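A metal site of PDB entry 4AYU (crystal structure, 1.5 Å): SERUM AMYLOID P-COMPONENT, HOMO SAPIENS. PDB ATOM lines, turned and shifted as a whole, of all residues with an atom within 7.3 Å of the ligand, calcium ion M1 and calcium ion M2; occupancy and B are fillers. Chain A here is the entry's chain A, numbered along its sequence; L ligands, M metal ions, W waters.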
ATOM      1  N   ALA A  46     -26.099  18.391  22.889  1.00  0.00           N
ATOM      2  CA  ALA A  46     -25.758  17.030  23.268  1.00  0.00           C
ATOM      3  C   ALA A  46     -26.972  16.124  23.169  1.00  0.00           C
ATOM      4  O   ALA A  46     -28.123  16.564  23.297  1.00  0.00           O
ATOM      5  CB  ALA A  46     -25.202  17.010  24.695  1.00  0.00           C
ATOM      6  N   TYR A  47     -26.730  14.848  22.950  1.00  0.00           N
ATOM      7  CA  TYR A  47     -27.801  13.873  22.892  1.00  0.00           C
ATOM      8  C   TYR A  47     -27.309  12.459  23.091  1.00  0.00           C
ATOM      9  O   TYR A  47     -26.174  12.144  22.786  1.00  0.00           O
ATOM     10  CB  TYR A  47     -28.579  13.992  21.568  1.00  0.00           C
ATOM     11  CG  TYR A  47     -27.775  13.908  20.285  1.00  0.00           C
ATOM     12  CD1 TYR A  47     -27.480  12.698  19.700  1.00  0.00           C
ATOM     13  CD2 TYR A  47     -27.386  15.064  19.629  1.00  0.00           C
ATOM     14  CE1 TYR A  47     -26.784  12.632  18.497  1.00  0.00           C
ATOM     15  CE2 TYR A  47     -26.693  15.003  18.434  1.00  0.00           C
ATOM     16  CZ  TYR A  47     -26.404  13.791  17.862  1.00  0.00           C
ATOM     17  OH  TYR A  47     -25.709  13.724  16.659  1.00  0.00           O
ATOM     18  N   SER A  48     -28.194  11.602  23.581  1.00  0.00           N
ATOM     19  CA  SER A  48     -27.929  10.195  23.719  1.00  0.00           C
ATOM     20  C   SER A  48     -28.173   9.440  22.402  1.00  0.00           C
ATOM     21  O   SER A  48     -29.235   9.599  21.762  1.00  0.00           O
ATOM     22  CB  SER A  48     -28.831   9.592  24.804  1.00  0.00           C
ATOM     23  OG  SER A  48     -28.603   8.207  24.916  1.00  0.00           O
ATOM     24  N   SER A  51     -28.683   4.097  24.930  1.00  0.00           N
ATOM     25  CA  SER A  51     -28.771   4.160  26.393  1.00  0.00           C
ATOM     26  C   SER A  51     -29.121   2.769  26.933  1.00  0.00           C
ATOM     27  O   SER A  51     -30.185   2.240  26.623  1.00  0.00           O
ATOM     28  CB  SER A  51     -29.839   5.178  26.787  1.00  0.00           C
ATOM     29  OG  SER A  51     -30.143   5.160  28.178  1.00  0.00           O
ATOM     30  N   ASN A  53     -29.306   0.847  30.574  1.00  0.00           N
ATOM     31  CA  ASN A  53     -29.351   0.956  32.031  1.00  0.00           C
ATOM     32  C   ASN A  53     -29.764  -0.389  32.608  1.00  0.00           C
ATOM     33  O   ASN A  53     -30.471  -1.169  31.979  1.00  0.00           O
ATOM     34  CB  ASN A  53     -30.376   2.016  32.460  1.00  0.00           C
ATOM     35  CG  ASN A  53     -29.797   3.420  32.541  1.00  0.00           C
ATOM     36  OD1 ASN A  53     -28.740   3.698  31.972  1.00  0.00           O
ATOM     37  ND2 ASN A  53     -30.508   4.307  33.244  1.00  0.00           N
ATOM     38  N   ASP A  58     -27.677   3.659  36.703  1.00  0.00           N
ATOM     39  CA  ASP A  58     -27.735   4.616  35.600  1.00  0.00           C
ATOM     40  C   ASP A  58     -26.432   4.586  34.817  1.00  0.00           C
ATOM     41  O   ASP A  58     -25.388   4.245  35.350  1.00  0.00           O
ATOM     42  CB  ASP A  58     -27.986   6.019  36.141  1.00  0.00           C
ATOM     43  CG  ASP A  58     -28.289   7.021  35.059  1.00  0.00           C
ATOM     44  OD1 ASP A  58     -28.909   6.608  34.043  1.00  0.00           O
ATOM     45  OD2 ASP A  58     -27.932   8.220  35.198  1.00  0.00           O
ATOM     46  N   ASN A  59     -26.514   4.919  33.532  1.00  0.00           N
ATOM     47  CA  ASN A  59     -25.331   5.078  32.696  1.00  0.00           C
ATOM     48  C   ASN A  59     -24.436   3.858  32.735  1.00  0.00           C
ATOM     49  O   ASN A  59     -23.211   3.961  32.822  1.00  0.00           O
ATOM     50  CB  ASN A  59     -24.543   6.320  33.099  1.00  0.00           C
ATOM     51  CG  ASN A  59     -25.394   7.568  33.017  1.00  0.00           C
ATOM     52  OD1 ASN A  59     -26.465   7.546  32.411  1.00  0.00           O
ATOM     53  ND2 ASN A  59     -24.933   8.650  33.616  1.00  0.00           N
ATOM     54  N   GLU A  60     -25.051   2.694  32.656  1.00  0.00           N
ATOM     55  CA  GLU A  60     -24.315   1.447  32.752  1.00  0.00           C
ATOM     56  C   GLU A  60     -23.526   1.203  31.461  1.00  0.00           C
ATOM     57  O   GLU A  60     -22.378   0.748  31.505  1.00  0.00           O
ATOM     58  CB  GLU A  60     -25.264   0.298  33.085  1.00  0.00           C
ATOM     59  CG  GLU A  60     -24.581  -1.040  33.264  1.00  0.00           C
ATOM     60  CD  GLU A  60     -23.667  -1.105  34.481  1.00  0.00           C
ATOM     61  OE1 GLU A  60     -23.702  -0.182  35.301  1.00  0.00           O
ATOM     62  OE2 GLU A  60     -22.913  -2.074  34.593  1.00  0.00           O
ATOM     63  N   LEU A  62     -23.506   3.706  27.886  1.00  0.00           N
ATOM     64  CA  LEU A  62     -24.147   4.833  27.227  1.00  0.00           C
ATOM     65  C   LEU A  62     -23.230   5.449  26.188  1.00  0.00           C
ATOM     66  O   LEU A  62     -22.072   5.791  26.466  1.00  0.00           O
ATOM     67  CB  LEU A  62     -24.549   5.903  28.248  1.00  0.00           C
ATOM     68  CG  LEU A  62     -24.924   7.291  27.728  1.00  0.00           C
ATOM     69  CD1 LEU A  62     -26.241   7.261  26.954  1.00  0.00           C
ATOM     70  CD2 LEU A  62     -25.022   8.298  28.896  1.00  0.00           C
ATOM     71  N   TYR A  64     -22.949   8.678  23.968  1.00  0.00           N
ATOM     72  CA  TYR A  64     -23.484  10.017  24.156  1.00  0.00           C
ATOM     73  C   TYR A  64     -22.693  10.991  23.296  1.00  0.00           C
ATOM     74  O   TYR A  64     -21.453  11.000  23.339  1.00  0.00           O
ATOM     75  CB  TYR A  64     -23.358  10.418  25.616  1.00  0.00           C
ATOM     76  CG  TYR A  64     -24.080  11.682  26.035  1.00  0.00           C
ATOM     77  CD1 TYR A  64     -25.458  11.693  26.173  1.00  0.00           C
ATOM     78  CD2 TYR A  64     -23.383  12.833  26.372  1.00  0.00           C
ATOM     79  CE1 TYR A  64     -26.121  12.819  26.592  1.00  0.00           C
ATOM     80  CE2 TYR A  64     -24.048  13.982  26.787  1.00  0.00           C
ATOM     81  CZ  TYR A  64     -25.413  13.962  26.901  1.00  0.00           C
ATOM     82  OH  TYR A  64     -26.117  15.072  27.342  1.00  0.00           O
ATOM     83  N   GLU A  66     -21.498  14.613  22.704  1.00  0.00           N
ATOM     84  CA  GLU A  66     -21.357  15.816  23.511  1.00  0.00           C
ATOM     85  C   GLU A  66     -21.621  17.104  22.719  1.00  0.00           C
ATOM     86  O   GLU A  66     -22.159  18.081  23.227  1.00  0.00           O
ATOM     87  CB  GLU A  66     -19.924  15.909  24.066  1.00  0.00           C
ATOM     88  CG  GLU A  66     -19.457  14.703  24.864  1.00  0.00           C
ATOM     89  CD  GLU A  66     -20.040  14.624  26.249  1.00  0.00           C
ATOM     90  OE1 GLU A  66     -20.675  15.607  26.698  1.00  0.00           O
ATOM     91  OE2 GLU A  66     -19.852  13.582  26.901  1.00  0.00           O
ATOM     92  N   TYR A  74     -19.903   5.881  28.191  1.00  0.00           N
ATOM     93  CA  TYR A  74     -19.937   5.599  29.618  1.00  0.00           C
ATOM     94  C   TYR A  74     -20.000   4.091  29.813  1.00  0.00           C
ATOM     95  O   TYR A  74     -20.759   3.420  29.131  1.00  0.00           O
ATOM     96  CB  TYR A  74     -21.172   6.212  30.300  1.00  0.00           C
ATOM     97  CG  TYR A  74     -21.229   7.720  30.392  1.00  0.00           C
ATOM     98  CD1 TYR A  74     -21.374   8.508  29.253  1.00  0.00           C
ATOM     99  CD2 TYR A  74     -21.189   8.367  31.622  1.00  0.00           C
ATOM    100  CE1 TYR A  74     -21.468   9.873  29.345  1.00  0.00           C
ATOM    101  CE2 TYR A  74     -21.268   9.731  31.706  1.00  0.00           C
ATOM    102  CZ  TYR A  74     -21.404  10.473  30.563  1.00  0.00           C
ATOM    103  OH  TYR A  74     -21.491  11.840  30.643  1.00  0.00           O
ATOM    104  N   LYS A  79     -16.725   7.636  32.303  1.00  0.00           N
ATOM    105  CA  LYS A  79     -16.785   8.005  30.888  1.00  0.00           C
ATOM    106  C   LYS A  79     -15.424   8.265  30.274  1.00  0.00           C
ATOM    107  O   LYS A  79     -14.456   8.657  30.959  1.00  0.00           O
ATOM    108  CB  LYS A  79     -17.672   9.230  30.662  1.00  0.00           C
ATOM    109  CG  LYS A  79     -17.061  10.513  31.133  1.00  0.00           C
ATOM    110  CD  LYS A  79     -18.013  11.711  31.030  1.00  0.00           C
ATOM    111  CE  LYS A  79     -18.359  12.061  29.604  1.00  0.00           C
ATOM    112  NZ  LYS A  79     -19.197  13.319  29.507  1.00  0.00           N
ATOM    113  N   GLU A 136     -32.295   9.416  26.708  1.00  0.00           N
ATOM    114  CA  GLU A 136     -31.298   9.019  27.689  1.00  0.00           C
ATOM    115  C   GLU A 136     -32.025   8.608  28.970  1.00  0.00           C
ATOM    116  O   GLU A 136     -32.781   9.395  29.516  1.00  0.00           O
ATOM    117  CB  GLU A 136     -30.360  10.202  27.952  1.00  0.00           C
ATOM    118  CG  GLU A 136     -28.975   9.801  28.430  1.00  0.00           C
ATOM    119  CD  GLU A 136     -28.921   9.419  29.889  1.00  0.00           C
ATOM    120  OE1 GLU A 136     -29.567  10.116  30.704  1.00  0.00           O
ATOM    121  OE2 GLU A 136     -28.245   8.426  30.219  1.00  0.00           O
ATOM    122  N   GLN A 137     -31.818   7.378  29.419  1.00  0.00           N
ATOM    123  CA  GLN A 137     -32.470   6.914  30.659  1.00  0.00           C
ATOM    124  C   GLN A 137     -31.758   7.457  31.875  1.00  0.00           C
ATOM    125  O   GLN A 137     -30.544   7.481  31.888  1.00  0.00           O
ATOM    126  CB  GLN A 137     -32.436   5.402  30.762  1.00  0.00           C
ATOM    127  CG  GLN A 137     -33.192   4.649  29.713  1.00  0.00           C
ATOM    128  CD  GLN A 137     -32.908   3.161  29.762  1.00  0.00           C
ATOM    129  OE1 GLN A 137     -33.523   2.416  30.531  1.00  0.00           O
ATOM    130  NE2 GLN A 137     -31.958   2.723  28.950  1.00  0.00           N
ATOM    131  N   ASP A 138     -32.513   7.831  32.901  1.00  0.00           N
ATOM    132  CA  ASP A 138     -31.948   8.021  34.250  1.00  0.00           C
ATOM    133  C   ASP A 138     -32.475   7.007  35.253  1.00  0.00           C
ATOM    134  O   ASP A 138     -32.032   6.982  36.400  1.00  0.00           O
ATOM    135  CB  ASP A 138     -32.195   9.437  34.746  1.00  0.00           C
ATOM    136  CG  ASP A 138     -31.354  10.464  34.028  1.00  0.00           C
ATOM    137  OD1 ASP A 138     -30.269  10.108  33.525  1.00  0.00           O
ATOM    138  OD2 ASP A 138     -31.756  11.656  33.982  1.00  0.00           O
ATOM    139  N   SER A 139     -33.432   6.182  34.840  1.00  0.00           N
ATOM    140  CA  SER A 139     -33.935   5.086  35.657  1.00  0.00           C
ATOM    141  C   SER A 139     -33.927   3.808  34.834  1.00  0.00           C
ATOM    142  O   SER A 139     -33.452   3.797  33.701  1.00  0.00           O
ATOM    143  CB  SER A 139     -35.356   5.397  36.115  1.00  0.00           C
ATOM    144  OG  SER A 139     -36.234   5.349  34.999  1.00  0.00           O
ATOM    145  N   GLY A 142     -36.686   4.548  32.118  1.00  0.00           N
ATOM    146  CA  GLY A 142     -37.341   5.838  32.054  1.00  0.00           C
ATOM    147  C   GLY A 142     -36.522   7.002  32.569  1.00  0.00           C
ATOM    148  O   GLY A 142     -35.293   6.998  32.469  1.00  0.00           O
ATOM    149  N   LYS A 143     -37.228   8.003  33.097  1.00  0.00           N
ATOM    150  CA  LYS A 143     -36.660   9.258  33.586  1.00  0.00           C
ATOM    151  C   LYS A 143     -35.816   9.895  32.498  1.00  0.00           C
ATOM    152  O   LYS A 143     -34.620  10.169  32.685  1.00  0.00           O
ATOM    153  CB  LYS A 143     -35.880   9.054  34.894  1.00  0.00           C
ATOM    154  CG  LYS A 143     -36.784   8.748  36.088  1.00  0.00           C
ATOM    155  CD  LYS A 143     -37.627   9.954  36.473  1.00  0.00           C
ATOM    156  CE  LYS A 143     -38.431   9.674  37.741  1.00  0.00           C
ATOM    157  NZ  LYS A 143     -39.384  10.776  38.064  1.00  0.00           N
ATOM    158  N   PHE A 144     -36.476  10.174  31.388  1.00  0.00           N
ATOM    159  CA  PHE A 144     -35.868  10.789  30.219  1.00  0.00           C
ATOM    160  C   PHE A 144     -35.734  12.296  30.419  1.00  0.00           C
ATOM    161  O   PHE A 144     -36.243  12.870  31.384  1.00  0.00           O
ATOM    162  CB  PHE A 144     -36.722  10.488  28.983  1.00  0.00           C
ATOM    163  CG  PHE A 144     -36.945   9.027  28.712  1.00  0.00           C
ATOM    164  CD1 PHE A 144     -35.939   8.098  28.911  1.00  0.00           C
ATOM    165  CD2 PHE A 144     -38.176   8.581  28.259  1.00  0.00           C
ATOM    166  CE1 PHE A 144     -36.143   6.767  28.645  1.00  0.00           C
ATOM    167  CE2 PHE A 144     -38.391   7.239  27.984  1.00  0.00           C
ATOM    168  CZ  PHE A 144     -37.362   6.331  28.176  1.00  0.00           C
ATOM    169  N   ASP A 145     -35.037  12.944  29.479  1.00  0.00           N
ATOM    170  CA  ASP A 145     -34.722  14.367  29.554  1.00  0.00           C
ATOM    171  C   ASP A 145     -34.748  14.915  28.128  1.00  0.00           C
ATOM    172  O   ASP A 145     -33.918  14.537  27.289  1.00  0.00           O
ATOM    173  CB  ASP A 145     -33.346  14.539  30.200  1.00  0.00           C
ATOM    174  CG  ASP A 145     -32.877  15.994  30.275  1.00  0.00           C
ATOM    175  OD1 ASP A 145     -33.488  16.893  29.655  1.00  0.00           O
ATOM    176  OD2 ASP A 145     -31.855  16.227  30.935  1.00  0.00           O
ATOM    177  N   GLN A 148     -31.658  15.881  26.172  1.00  0.00           N
ATOM    178  CA  GLN A 148     -30.757  14.807  25.765  1.00  0.00           C
ATOM    179  C   GLN A 148     -31.394  13.895  24.723  1.00  0.00           C
ATOM    180  O   GLN A 148     -30.789  12.884  24.333  1.00  0.00           O
ATOM    181  CB  GLN A 148     -30.339  13.986  26.972  1.00  0.00           C
ATOM    182  CG  GLN A 148     -29.619  14.793  28.035  1.00  0.00           C
ATOM    183  CD  GLN A 148     -29.239  13.971  29.268  1.00  0.00           C
ATOM    184  OE1 GLN A 148     -30.050  13.235  29.811  1.00  0.00           O
ATOM    185  NE2 GLN A 148     -27.998  14.107  29.699  1.00  0.00           N
HETATM  186  C1  LIG L   1     -25.435  14.472  32.526  1.00  0.00           C
HETATM  187  O1  LIG L   1     -25.191  15.591  32.052  1.00  0.00           O
HETATM  188  C2  LIG L   1     -25.912  14.310  33.925  1.00  0.00           C
HETATM  189  N1  LIG L   1     -25.266  13.309  31.723  1.00  0.00           N
HETATM  190  C3  LIG L   1     -25.500  11.965  32.166  1.00  0.00           C
HETATM  191  C4  LIG L   1     -24.941  11.088  31.087  1.00  0.00           C
HETATM  192  C5  LIG L   1     -24.993  11.902  29.858  1.00  0.00           C
HETATM  193  C6  LIG L   1     -24.795  13.322  30.349  1.00  0.00           C
HETATM  194  C7  LIG L   1     -26.943  11.629  32.421  1.00  0.00           C
HETATM  195  O2  LIG L   1     -27.854  12.410  32.015  1.00  0.00           O
HETATM  196  O3  LIG L   1     -27.229  10.566  33.033  1.00  0.00           O
HETATM  197 CA    CA M   1     -30.203  12.058  31.934  1.00  0.00          CA
HETATM  198 CA    CA M   2     -28.600   8.653  32.636  1.00  0.00          CA
HETATM  199  O   HOH W   1     -30.753  14.349  32.480  1.00  0.00           O
HETATM  200  O   HOH W   2     -32.471  11.469  31.215  1.00  0.00           O
HETATM  201  O   HOH W   3     -28.601  11.337  36.082  1.00  0.00           O
HETATM  202  O   HOH W   4     -29.110  13.148  34.188  1.00  0.00           O
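An oxygen (O2) of the ligand is bound to calcium ion M1, at 2.4 Å.
OE1 of Glu 136 is bound to calcium ion M1 (2.4 Å).
Calcium ion M1 is bound by water W1 (2.4 Å).
Calcium ion M1 is bound by OE1 of Gln 148 (2.4 Å).
Calcium ion M1 is bound by water W2.
Calcium ion M1 is bound by OD1 of Asp 138, 2.5 Å away.
OD2 of Asp 138 is bound to calcium ion M1 (2.6 Å).
Water W4 binds calcium ion M1 (2.7 Å).
Calcium ion M1 has eight donor atoms within binding distance.
Calcium ion M2 is bound by the side-chain carboxylate (OD1) of Asp 138 (2.4 Å), an oxygen (O3) of the ligand (2.4 Å), the backbone carbonyl oxygen (O) of Gln 137 (2.4 Å), the side-chain amide oxygen (OD1) of Asn 59 (2.4 Å), the side-chain carboxylate (OE2) of Glu 136 (2.5 Å), the side-chain carboxylate (OD1) of Asp 58 (2.5 Å), the side-chain carboxylate (OE1) of Glu 136 (2.6 Å) and the side-chain carboxylate (OD2) of Asp 58 (2.7 Å).
Calcium ion M2 has eight donor atoms within binding distance.
Residues that only touch the ligand: Leu 62 (3.5 Å), Tyr 74 (3.6 Å) and Tyr 64 (3.6 Å).
The nearest printed residue that does not touch the ligand is Gln 137 (4.7 Å).
N of Asp 138 lies within hydrogen-bond range of O of Lys 143 (3.2 Å).
The side-chain amide nitrogen of Asn 53 lies close to the backbone carbonyl oxygen of Gln 137 (3.5 Å).
The backbone carbonyl oxygen (O) of Ser 51 is in hydrogen-bond range of the side-chain amide nitrogen (NE2) of Gln 137.
The backbone NH of Asn 59 sits at hydrogen-bond distance from the side-chain amide oxygen of Asn 53.
NE2 of Gln 148 sits at hydrogen-bond distance from OH of Tyr 64 (3.2 Å).
The backbone carbonyl oxygen (O) of Gln 148 lies within hydrogen-bond range of the backbone NH (N) of Ser 48 (3.0 Å).
The side-chain amide nitrogen (ND2) of Asn 53 sits close to the side-chain carboxylate (OD1) of Asp 58 (2.9 Å).
OH of Tyr 74 sits at hydrogen-bond distance from NZ of Lys 79 (3.0 Å).
Of the 22 residues printed, 3 come within 4 Å of calcium ion M1.
Water W2 lies within hydrogen-bond range of the backbone carbonyl oxygen of Glu 136 (2.7 Å), the backbone carbonyl oxygen of Lys 143 (2.9 Å) and the backbone NH of Asp 145 (3.4 Å).
Within 4 Å of calcium ion M2: Asp 58, Asn 59, Glu 136, Gln 137 and Asp 138.
The nearest printed residue that does not touch calcium ion M2 is Asn 53 (4.8 Å).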
